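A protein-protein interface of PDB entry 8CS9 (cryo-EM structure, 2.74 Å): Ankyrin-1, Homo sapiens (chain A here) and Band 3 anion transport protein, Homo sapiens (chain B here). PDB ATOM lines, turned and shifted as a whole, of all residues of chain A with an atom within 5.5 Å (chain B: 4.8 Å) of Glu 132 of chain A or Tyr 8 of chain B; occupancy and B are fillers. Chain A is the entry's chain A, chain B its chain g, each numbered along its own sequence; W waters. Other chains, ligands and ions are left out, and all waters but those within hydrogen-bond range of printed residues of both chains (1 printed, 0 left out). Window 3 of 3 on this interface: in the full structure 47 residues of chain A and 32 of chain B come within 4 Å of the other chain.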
ATOM      1  N   ARG A  95     -23.661 -23.391  33.335  1.00  0.00           N
ATOM      2  CA  ARG A  95     -22.610 -24.316  33.744  1.00  0.00           C
ATOM      3  C   ARG A  95     -23.129 -25.345  34.739  1.00  0.00           C
ATOM      4  O   ARG A  95     -22.857 -26.540  34.598  1.00  0.00           O
ATOM      5  CB  ARG A  95     -21.436 -23.541  34.340  1.00  0.00           C
ATOM      6  CG  ARG A  95     -20.319 -23.285  33.357  1.00  0.00           C
ATOM      7  CD  ARG A  95     -19.204 -22.447  33.957  1.00  0.00           C
ATOM      8  NE  ARG A  95     -18.061 -22.354  33.056  1.00  0.00           N
ATOM      9  CZ  ARG A  95     -18.050 -21.667  31.922  1.00  0.00           C
ATOM     10  NH1 ARG A  95     -19.106 -20.978  31.518  1.00  0.00           N
ATOM     11  NH2 ARG A  95     -16.951 -21.666  31.176  1.00  0.00           N
ATOM     12  N   VAL A 127     -22.100 -19.602  24.454  1.00  0.00           N
ATOM     13  CA  VAL A 127     -21.839 -20.283  23.187  1.00  0.00           C
ATOM     14  C   VAL A 127     -20.587 -21.143  23.296  1.00  0.00           C
ATOM     15  O   VAL A 127     -20.576 -22.308  22.883  1.00  0.00           O
ATOM     16  CB  VAL A 127     -21.723 -19.257  22.044  1.00  0.00           C
ATOM     17  CG1 VAL A 127     -21.037 -19.870  20.829  1.00  0.00           C
ATOM     18  CG2 VAL A 127     -23.088 -18.726  21.667  1.00  0.00           C
ATOM     19  N   LYS A 128     -19.521 -20.584  23.872  1.00  0.00           N
ATOM     20  CA  LYS A 128     -18.271 -21.322  24.016  1.00  0.00           C
ATOM     21  C   LYS A 128     -18.443 -22.539  24.916  1.00  0.00           C
ATOM     22  O   LYS A 128     -17.968 -23.633  24.586  1.00  0.00           O
ATOM     23  CB  LYS A 128     -17.182 -20.399  24.563  1.00  0.00           C
ATOM     24  CG  LYS A 128     -15.848 -21.087  24.811  1.00  0.00           C
ATOM     25  CD  LYS A 128     -14.852 -20.154  25.481  1.00  0.00           C
ATOM     26  CE  LYS A 128     -14.142 -19.267  24.469  1.00  0.00           C
ATOM     27  NZ  LYS A 128     -14.854 -17.975  24.250  1.00  0.00           N
ATOM     28  N   PHE A 129     -19.130 -22.375  26.050  1.00  0.00           N
ATOM     29  CA  PHE A 129     -19.334 -23.502  26.955  1.00  0.00           C
ATOM     30  C   PHE A 129     -20.202 -24.583  26.320  1.00  0.00           C
ATOM     31  O   PHE A 129     -19.914 -25.778  26.456  1.00  0.00           O
ATOM     32  CB  PHE A 129     -19.950 -23.021  28.267  1.00  0.00           C
ATOM     33  CG  PHE A 129     -20.092 -24.102  29.296  1.00  0.00           C
ATOM     34  CD1 PHE A 129     -18.988 -24.559  29.992  1.00  0.00           C
ATOM     35  CD2 PHE A 129     -21.325 -24.663  29.566  1.00  0.00           C
ATOM     36  CE1 PHE A 129     -19.112 -25.555  30.935  1.00  0.00           C
ATOM     37  CE2 PHE A 129     -21.455 -25.658  30.507  1.00  0.00           C
ATOM     38  CZ  PHE A 129     -20.350 -26.105  31.194  1.00  0.00           C
ATOM     39  N   LEU A 130     -21.264 -24.185  25.616  1.00  0.00           N
ATOM     40  CA  LEU A 130     -22.126 -25.160  24.962  1.00  0.00           C
ATOM     41  C   LEU A 130     -21.381 -25.913  23.870  1.00  0.00           C
ATOM     42  O   LEU A 130     -21.531 -27.134  23.741  1.00  0.00           O
ATOM     43  CB  LEU A 130     -23.362 -24.467  24.393  1.00  0.00           C
ATOM     44  CG  LEU A 130     -24.462 -24.135  25.400  1.00  0.00           C
ATOM     45  CD1 LEU A 130     -25.453 -23.162  24.799  1.00  0.00           C
ATOM     46  CD2 LEU A 130     -25.163 -25.399  25.866  1.00  0.00           C
ATOM     47  N   LEU A 131     -20.563 -25.209  23.082  1.00  0.00           N
ATOM     48  CA  LEU A 131     -19.756 -25.879  22.068  1.00  0.00           C
ATOM     49  C   LEU A 131     -18.769 -26.844  22.705  1.00  0.00           C
ATOM     50  O   LEU A 131     -18.572 -27.959  22.211  1.00  0.00           O
ATOM     51  CB  LEU A 131     -19.022 -24.850  21.211  1.00  0.00           C
ATOM     52  CG  LEU A 131     -19.861 -24.048  20.217  1.00  0.00           C
ATOM     53  CD1 LEU A 131     -19.019 -22.962  19.577  1.00  0.00           C
ATOM     54  CD2 LEU A 131     -20.470 -24.956  19.167  1.00  0.00           C
ATOM     55  N   GLU A 132     -18.142 -26.438  23.812  1.00  0.00           N
ATOM     56  CA  GLU A 132     -17.245 -27.329  24.535  1.00  0.00           C
ATOM     57  C   GLU A 132     -17.969 -28.513  25.157  1.00  0.00           C
ATOM     58  O   GLU A 132     -17.322 -29.517  25.466  1.00  0.00           O
ATOM     59  CB  GLU A 132     -16.498 -26.555  25.620  1.00  0.00           C
ATOM     60  CG  GLU A 132     -15.361 -25.692  25.101  1.00  0.00           C
ATOM     61  CD  GLU A 132     -14.869 -24.696  26.132  1.00  0.00           C
ATOM     62  OE1 GLU A 132     -15.285 -24.798  27.306  1.00  0.00           O
ATOM     63  OE2 GLU A 132     -14.066 -23.812  25.770  1.00  0.00           O
ATOM     64  N   ASN A 133     -19.286 -28.423  25.352  1.00  0.00           N
ATOM     65  CA  ASN A 133     -20.061 -29.523  25.911  1.00  0.00           C
ATOM     66  C   ASN A 133     -20.863 -30.271  24.851  1.00  0.00           C
ATOM     67  O   ASN A 133     -21.868 -30.910  25.175  1.00  0.00           O
ATOM     68  CB  ASN A 133     -20.981 -29.015  27.020  1.00  0.00           C
ATOM     69  CG  ASN A 133     -20.225 -28.701  28.292  1.00  0.00           C
ATOM     70  OD1 ASN A 133     -20.172 -29.513  29.212  1.00  0.00           O
ATOM     71  ND2 ASN A 133     -19.622 -27.523  28.343  1.00  0.00           N
ATOM     72  N   GLY A 134     -20.433 -30.215  23.595  1.00  0.00           N
ATOM     73  CA  GLY A 134     -21.022 -31.043  22.562  1.00  0.00           C
ATOM     74  C   GLY A 134     -22.309 -30.541  21.953  1.00  0.00           C
ATOM     75  O   GLY A 134     -23.087 -31.348  21.440  1.00  0.00           O
ATOM     76  N   TYR A 166     -14.621 -22.997  15.872  1.00  0.00           N
ATOM     77  CA  TYR A 166     -14.857 -24.276  16.535  1.00  0.00           C
ATOM     78  C   TYR A 166     -15.134 -25.379  15.522  1.00  0.00           C
ATOM     79  O   TYR A 166     -14.583 -26.480  15.628  1.00  0.00           O
ATOM     80  CB  TYR A 166     -16.016 -24.149  17.524  1.00  0.00           C
ATOM     81  CG  TYR A 166     -16.047 -25.235  18.573  1.00  0.00           C
ATOM     82  CD1 TYR A 166     -16.673 -26.449  18.325  1.00  0.00           C
ATOM     83  CD2 TYR A 166     -15.447 -25.048  19.811  1.00  0.00           C
ATOM     84  CE1 TYR A 166     -16.701 -27.444  19.278  1.00  0.00           C
ATOM     85  CE2 TYR A 166     -15.471 -26.039  20.770  1.00  0.00           C
ATOM     86  CZ  TYR A 166     -16.096 -27.233  20.499  1.00  0.00           C
ATOM     87  OH  TYR A 166     -16.122 -28.221  21.451  1.00  0.00           O
ATOM     88  N   GLY A 170     -16.392 -30.942  18.491  1.00  0.00           N
ATOM     89  CA  GLY A 170     -17.125 -31.835  19.361  1.00  0.00           C
ATOM     90  C   GLY A 170     -16.956 -31.499  20.834  1.00  0.00           C
ATOM     91  O   GLY A 170     -16.506 -30.422  21.223  1.00  0.00           O
ATOM     92  N   LYS A 171     -17.334 -32.470  21.660  1.00  0.00           N
ATOM     93  CA  LYS A 171     -17.260 -32.312  23.108  1.00  0.00           C
ATOM     94  C   LYS A 171     -15.813 -32.445  23.567  1.00  0.00           C
ATOM     95  O   LYS A 171     -15.243 -33.539  23.542  1.00  0.00           O
ATOM     96  CB  LYS A 171     -18.147 -33.348  23.792  1.00  0.00           C
ATOM     97  CG  LYS A 171     -18.633 -32.928  25.165  1.00  0.00           C
ATOM     98  CD  LYS A 171     -19.561 -33.961  25.766  1.00  0.00           C
ATOM     99  CE  LYS A 171     -19.617 -33.832  27.277  1.00  0.00           C
ATOM    100  NZ  LYS A 171     -20.148 -35.063  27.918  1.00  0.00           N
ATOM    101  N   VAL A 172     -15.217 -31.331  23.986  1.00  0.00           N
ATOM    102  CA  VAL A 172     -13.869 -31.325  24.540  1.00  0.00           C
ATOM    103  C   VAL A 172     -13.872 -31.228  26.052  1.00  0.00           C
ATOM    104  O   VAL A 172     -12.796 -31.222  26.665  1.00  0.00           O
ATOM    105  CB  VAL A 172     -13.017 -30.199  23.931  1.00  0.00           C
ATOM    106  CG1 VAL A 172     -12.750 -30.486  22.466  1.00  0.00           C
ATOM    107  CG2 VAL A 172     -13.703 -28.859  24.104  1.00  0.00           C
ATOM    108  N   ARG A 173     -15.041 -31.145  26.674  1.00  0.00           N
ATOM    109  CA  ARG A 173     -15.167 -31.212  28.119  1.00  0.00           C
ATOM    110  C   ARG A 173     -15.523 -32.632  28.534  1.00  0.00           C
ATOM    111  O   ARG A 173     -16.126 -33.390  27.771  1.00  0.00           O
ATOM    112  CB  ARG A 173     -16.228 -30.238  28.631  1.00  0.00           C
ATOM    113  CG  ARG A 173     -15.802 -29.468  29.866  1.00  0.00           C
ATOM    114  CD  ARG A 173     -16.875 -28.501  30.314  1.00  0.00           C
ATOM    115  NE  ARG A 173     -17.989 -29.182  30.960  1.00  0.00           N
ATOM    116  CZ  ARG A 173     -18.372 -28.968  32.211  1.00  0.00           C
ATOM    117  NH1 ARG A 173     -17.744 -28.102  32.986  1.00  0.00           N
ATOM    118  NH2 ARG A 173     -19.409 -29.644  32.694  1.00  0.00           N
ATOM    119  N   LEU A 174     -15.140 -32.985  29.756  1.00  0.00           N
ATOM    120  CA  LEU A 174     -15.411 -34.309  30.277  1.00  0.00           C
ATOM    121  C   LEU A 174     -16.911 -34.504  30.483  1.00  0.00           C
ATOM    122  O   LEU A 174     -17.661 -33.533  30.605  1.00  0.00           O
ATOM    123  CB  LEU A 174     -14.670 -34.518  31.593  1.00  0.00           C
ATOM    124  CG  LEU A 174     -13.181 -34.844  31.499  1.00  0.00           C
ATOM    125  CD1 LEU A 174     -12.516 -34.587  32.832  1.00  0.00           C
ATOM    126  CD2 LEU A 174     -12.963 -36.281  31.054  1.00  0.00           C
ATOM    127  N   LEU B   4     -10.383 -24.776  36.792  1.00  0.00           N
ATOM    128  CA  LEU B   4     -11.347 -25.476  35.954  1.00  0.00           C
ATOM    129  C   LEU B   4     -10.694 -26.126  34.741  1.00  0.00           C
ATOM    130  O   LEU B   4     -11.404 -26.677  33.893  1.00  0.00           O
ATOM    131  CB  LEU B   4     -12.460 -24.526  35.494  1.00  0.00           C
ATOM    132  CG  LEU B   4     -13.445 -24.042  36.560  1.00  0.00           C
ATOM    133  CD1 LEU B   4     -14.362 -22.969  35.994  1.00  0.00           C
ATOM    134  CD2 LEU B   4     -14.252 -25.207  37.114  1.00  0.00           C
ATOM    135  N   GLN B   5      -9.364 -26.073  34.636  1.00  0.00           N
ATOM    136  CA  GLN B   5      -8.683 -26.686  33.500  1.00  0.00           C
ATOM    137  C   GLN B   5      -8.811 -28.202  33.516  1.00  0.00           C
ATOM    138  O   GLN B   5      -8.847 -28.829  32.451  1.00  0.00           O
ATOM    139  CB  GLN B   5      -7.211 -26.277  33.489  1.00  0.00           C
ATOM    140  N   ASP B   6      -8.901 -28.804  34.700  1.00  0.00           N
ATOM    141  CA  ASP B   6      -8.958 -30.254  34.837  1.00  0.00           C
ATOM    142  C   ASP B   6     -10.282 -30.851  34.375  1.00  0.00           C
ATOM    143  O   ASP B   6     -10.403 -32.079  34.330  1.00  0.00           O
ATOM    144  CB  ASP B   6      -8.691 -30.651  36.293  1.00  0.00           C
ATOM    145  N   ASP B   7     -11.271 -30.027  34.044  1.00  0.00           N
ATOM    146  CA  ASP B   7     -12.556 -30.504  33.553  1.00  0.00           C
ATOM    147  C   ASP B   7     -12.524 -30.903  32.083  1.00  0.00           C
ATOM    148  O   ASP B   7     -13.530 -31.397  31.569  1.00  0.00           O
ATOM    149  CB  ASP B   7     -13.633 -29.436  33.764  1.00  0.00           C
ATOM    150  CG  ASP B   7     -13.952 -29.207  35.227  1.00  0.00           C
ATOM    151  OD1 ASP B   7     -13.082 -29.480  36.079  1.00  0.00           O
ATOM    152  OD2 ASP B   7     -15.075 -28.751  35.523  1.00  0.00           O
ATOM    153  N   TYR B   8     -11.402 -30.709  31.400  1.00  0.00           N
ATOM    154  CA  TYR B   8     -11.312 -30.930  29.967  1.00  0.00           C
ATOM    155  C   TYR B   8     -10.523 -32.198  29.676  1.00  0.00           C
ATOM    156  O   TYR B   8      -9.660 -32.607  30.455  1.00  0.00           O
ATOM    157  CB  TYR B   8     -10.685 -29.722  29.263  1.00  0.00           C
ATOM    158  CG  TYR B   8     -11.511 -28.460  29.408  1.00  0.00           C
ATOM    159  CD1 TYR B   8     -11.733 -27.883  30.656  1.00  0.00           C
ATOM    160  CD2 TYR B   8     -12.097 -27.863  28.305  1.00  0.00           C
ATOM    161  CE1 TYR B   8     -12.498 -26.758  30.800  1.00  0.00           C
ATOM    162  CE2 TYR B   8     -12.865 -26.724  28.440  1.00  0.00           C
ATOM    163  CZ  TYR B   8     -13.061 -26.177  29.690  1.00  0.00           C
ATOM    164  OH  TYR B   8     -13.825 -25.042  29.832  1.00  0.00           O
ATOM    165  N   GLU B   9     -10.843 -32.824  28.541  1.00  0.00           N
ATOM    166  CA  GLU B   9     -10.339 -34.162  28.249  1.00  0.00           C
ATOM    167  C   GLU B   9      -8.828 -34.175  28.051  1.00  0.00           C
ATOM    168  O   GLU B   9      -8.155 -35.122  28.470  1.00  0.00           O
ATOM    169  CB  GLU B   9     -11.049 -34.731  27.023  1.00  0.00           C
ATOM    170  CG  GLU B   9     -12.559 -34.664  27.116  1.00  0.00           C
ATOM    171  CD  GLU B   9     -13.193 -36.028  27.270  1.00  0.00           C
ATOM    172  OE1 GLU B   9     -12.515 -36.945  27.773  1.00  0.00           O
ATOM    173  OE2 GLU B   9     -14.376 -36.182  26.901  1.00  0.00           O
ATOM    174  N   ASP B  10      -8.278 -33.148  27.401  1.00  0.00           N
ATOM    175  CA  ASP B  10      -6.833 -33.101  27.200  1.00  0.00           C
ATOM    176  C   ASP B  10      -6.092 -32.974  28.526  1.00  0.00           C
ATOM    177  O   ASP B  10      -5.110 -33.689  28.770  1.00  0.00           O
ATOM    178  CB  ASP B  10      -6.469 -31.946  26.268  1.00  0.00           C
ATOM    179  CG  ASP B  10      -7.054 -32.108  24.881  1.00  0.00           C
ATOM    180  OD1 ASP B  10      -7.425 -33.245  24.520  1.00  0.00           O
ATOM    181  OD2 ASP B  10      -7.141 -31.100  24.151  1.00  0.00           O
ATOM    182  N   MET B  11      -6.559 -32.083  29.401  1.00  0.00           N
ATOM    183  CA  MET B  11      -5.905 -31.906  30.692  1.00  0.00           C
ATOM    184  C   MET B  11      -6.048 -33.147  31.560  1.00  0.00           C
ATOM    185  O   MET B  11      -5.118 -33.511  32.283  1.00  0.00           O
ATOM    186  CB  MET B  11      -6.467 -30.684  31.410  1.00  0.00           C
ATOM    187  CG  MET B  11      -5.533 -30.111  32.461  1.00  0.00           C
ATOM    188  SD  MET B  11      -3.802 -30.206  31.970  1.00  0.00           S
ATOM    189  CE  MET B  11      -3.184 -28.650  32.606  1.00  0.00           C
ATOM    190  N   MET B  12      -7.203 -33.811  31.505  1.00  0.00           N
ATOM    191  CA  MET B  12      -7.384 -35.019  32.302  1.00  0.00           C
ATOM    192  C   MET B  12      -6.531 -36.163  31.766  1.00  0.00           C
ATOM    193  O   MET B  12      -6.016 -36.980  32.535  1.00  0.00           O
ATOM    194  CB  MET B  12      -8.861 -35.407  32.347  1.00  0.00           C
ATOM    195  CG  MET B  12      -9.158 -36.525  33.331  1.00  0.00           C
ATOM    196  SD  MET B  12      -8.833 -36.002  35.026  1.00  0.00           S
ATOM    197  CE  MET B  12     -10.493 -35.739  35.642  1.00  0.00           C
HETATM  198  O   HOH W   1      -9.716 -30.421  25.598  1.00  0.00           O
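The backbone carbonyl oxygen (O) of Arg 173 of chain A lies close to the side-chain carboxylate (OE2) of Glu 9 of chain B, at 3.4 Å. The side-chain hydroxyl (OH) of Tyr 8 of chain B lies within hydrogen-bond range of the side-chain carboxylate (OE1) of Glu 132 of chain A (2.9 Å). The backbone carbonyl oxygen (O) of Val 172 of chain A is in hydrogen-bond range of the backbone NH (N) of Glu 9 of chain B, at 3.1 Å. The backbone NH (N) of Leu 174 of chain A is in hydrogen-bond range of the backbone carbonyl oxygen (O) of Asp 7 of chain B, at 2.9 Å. The guanidinium group (NH1) of Arg 173 of chain A is in salt-bridge range of the side-chain carboxylate (OD2) of Asp 7 of chain B, 3.7 Å away.
O of Glu 132 of chain A sits at hydrogen-bond distance from N of Arg 173 of chain A (3.1 Å). The guanidinium group of Arg 173 of chain A lies within hydrogen-bond range of the side-chain amide oxygen of Asn 133 of chain A (2.8 Å). O of Glu 132 of chain A lies within hydrogen-bond range of N of Val 172 of chain A (3.1 Å).
Among the printed residues, merely in contact across the chains: Leu 174 of chain A with Glu 9 of chain B (3.4 Å), Leu 174 of chain A with Asp 6 of chain B (3.6 Å), Val 172 of chain A with Tyr 8 of chain B (3.6 Å) and Leu 174 of chain A with Met 12 of chain B (3.6 Å).
Of chain B, only Tyr 8 (2.9 Å) comes within 4 Å of Glu 132 of chain A. Of the printed residues of chain B, Val 172 of chain A touches Tyr 8 (3.6 Å) and Glu 9 (3.1 Å). Printed residues of chain A within 4 Å of Asp 7 of chain B: Arg 173 and Leu 174. Tyr 8 of chain B touches just these residues of chain A: Glu 132 and Val 172. Of the printed residues of chain A, Glu 9 of chain B touches Val 172 (3.1 Å), Arg 173 (3.4 Å) and Leu 174 (3.4 Å). Of the printed residues of chain A, Met 12 of chain B touches Leu 174 (3.6 Å). The nearest residue of chain A that does not touch Tyr 8 of chain B is Leu 174 of chain A (4.2 Å).
Printed residues of chain B that touch a printed residue of chain A: Asp 6, Asp 7, Tyr 8, Glu 9 and Met 12. Hydrophobic or aromatic side chains of chain B within 4 Å of the printed part of chain A: Tyr 8 and Met 12. Among the printed residues, Asp or Glu carboxylates within 4 Å of a Lys or Arg side-chain nitrogen of the other chain: Arg 173 of chain A with Asp 7 of chain B.
Water W1 bridges the side-chain carboxylate (OD2) of Asp 10 of chain B (3.0 Å) and the backbone carbonyl oxygen (O) of Val 172 of chain A (3.4 Å).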
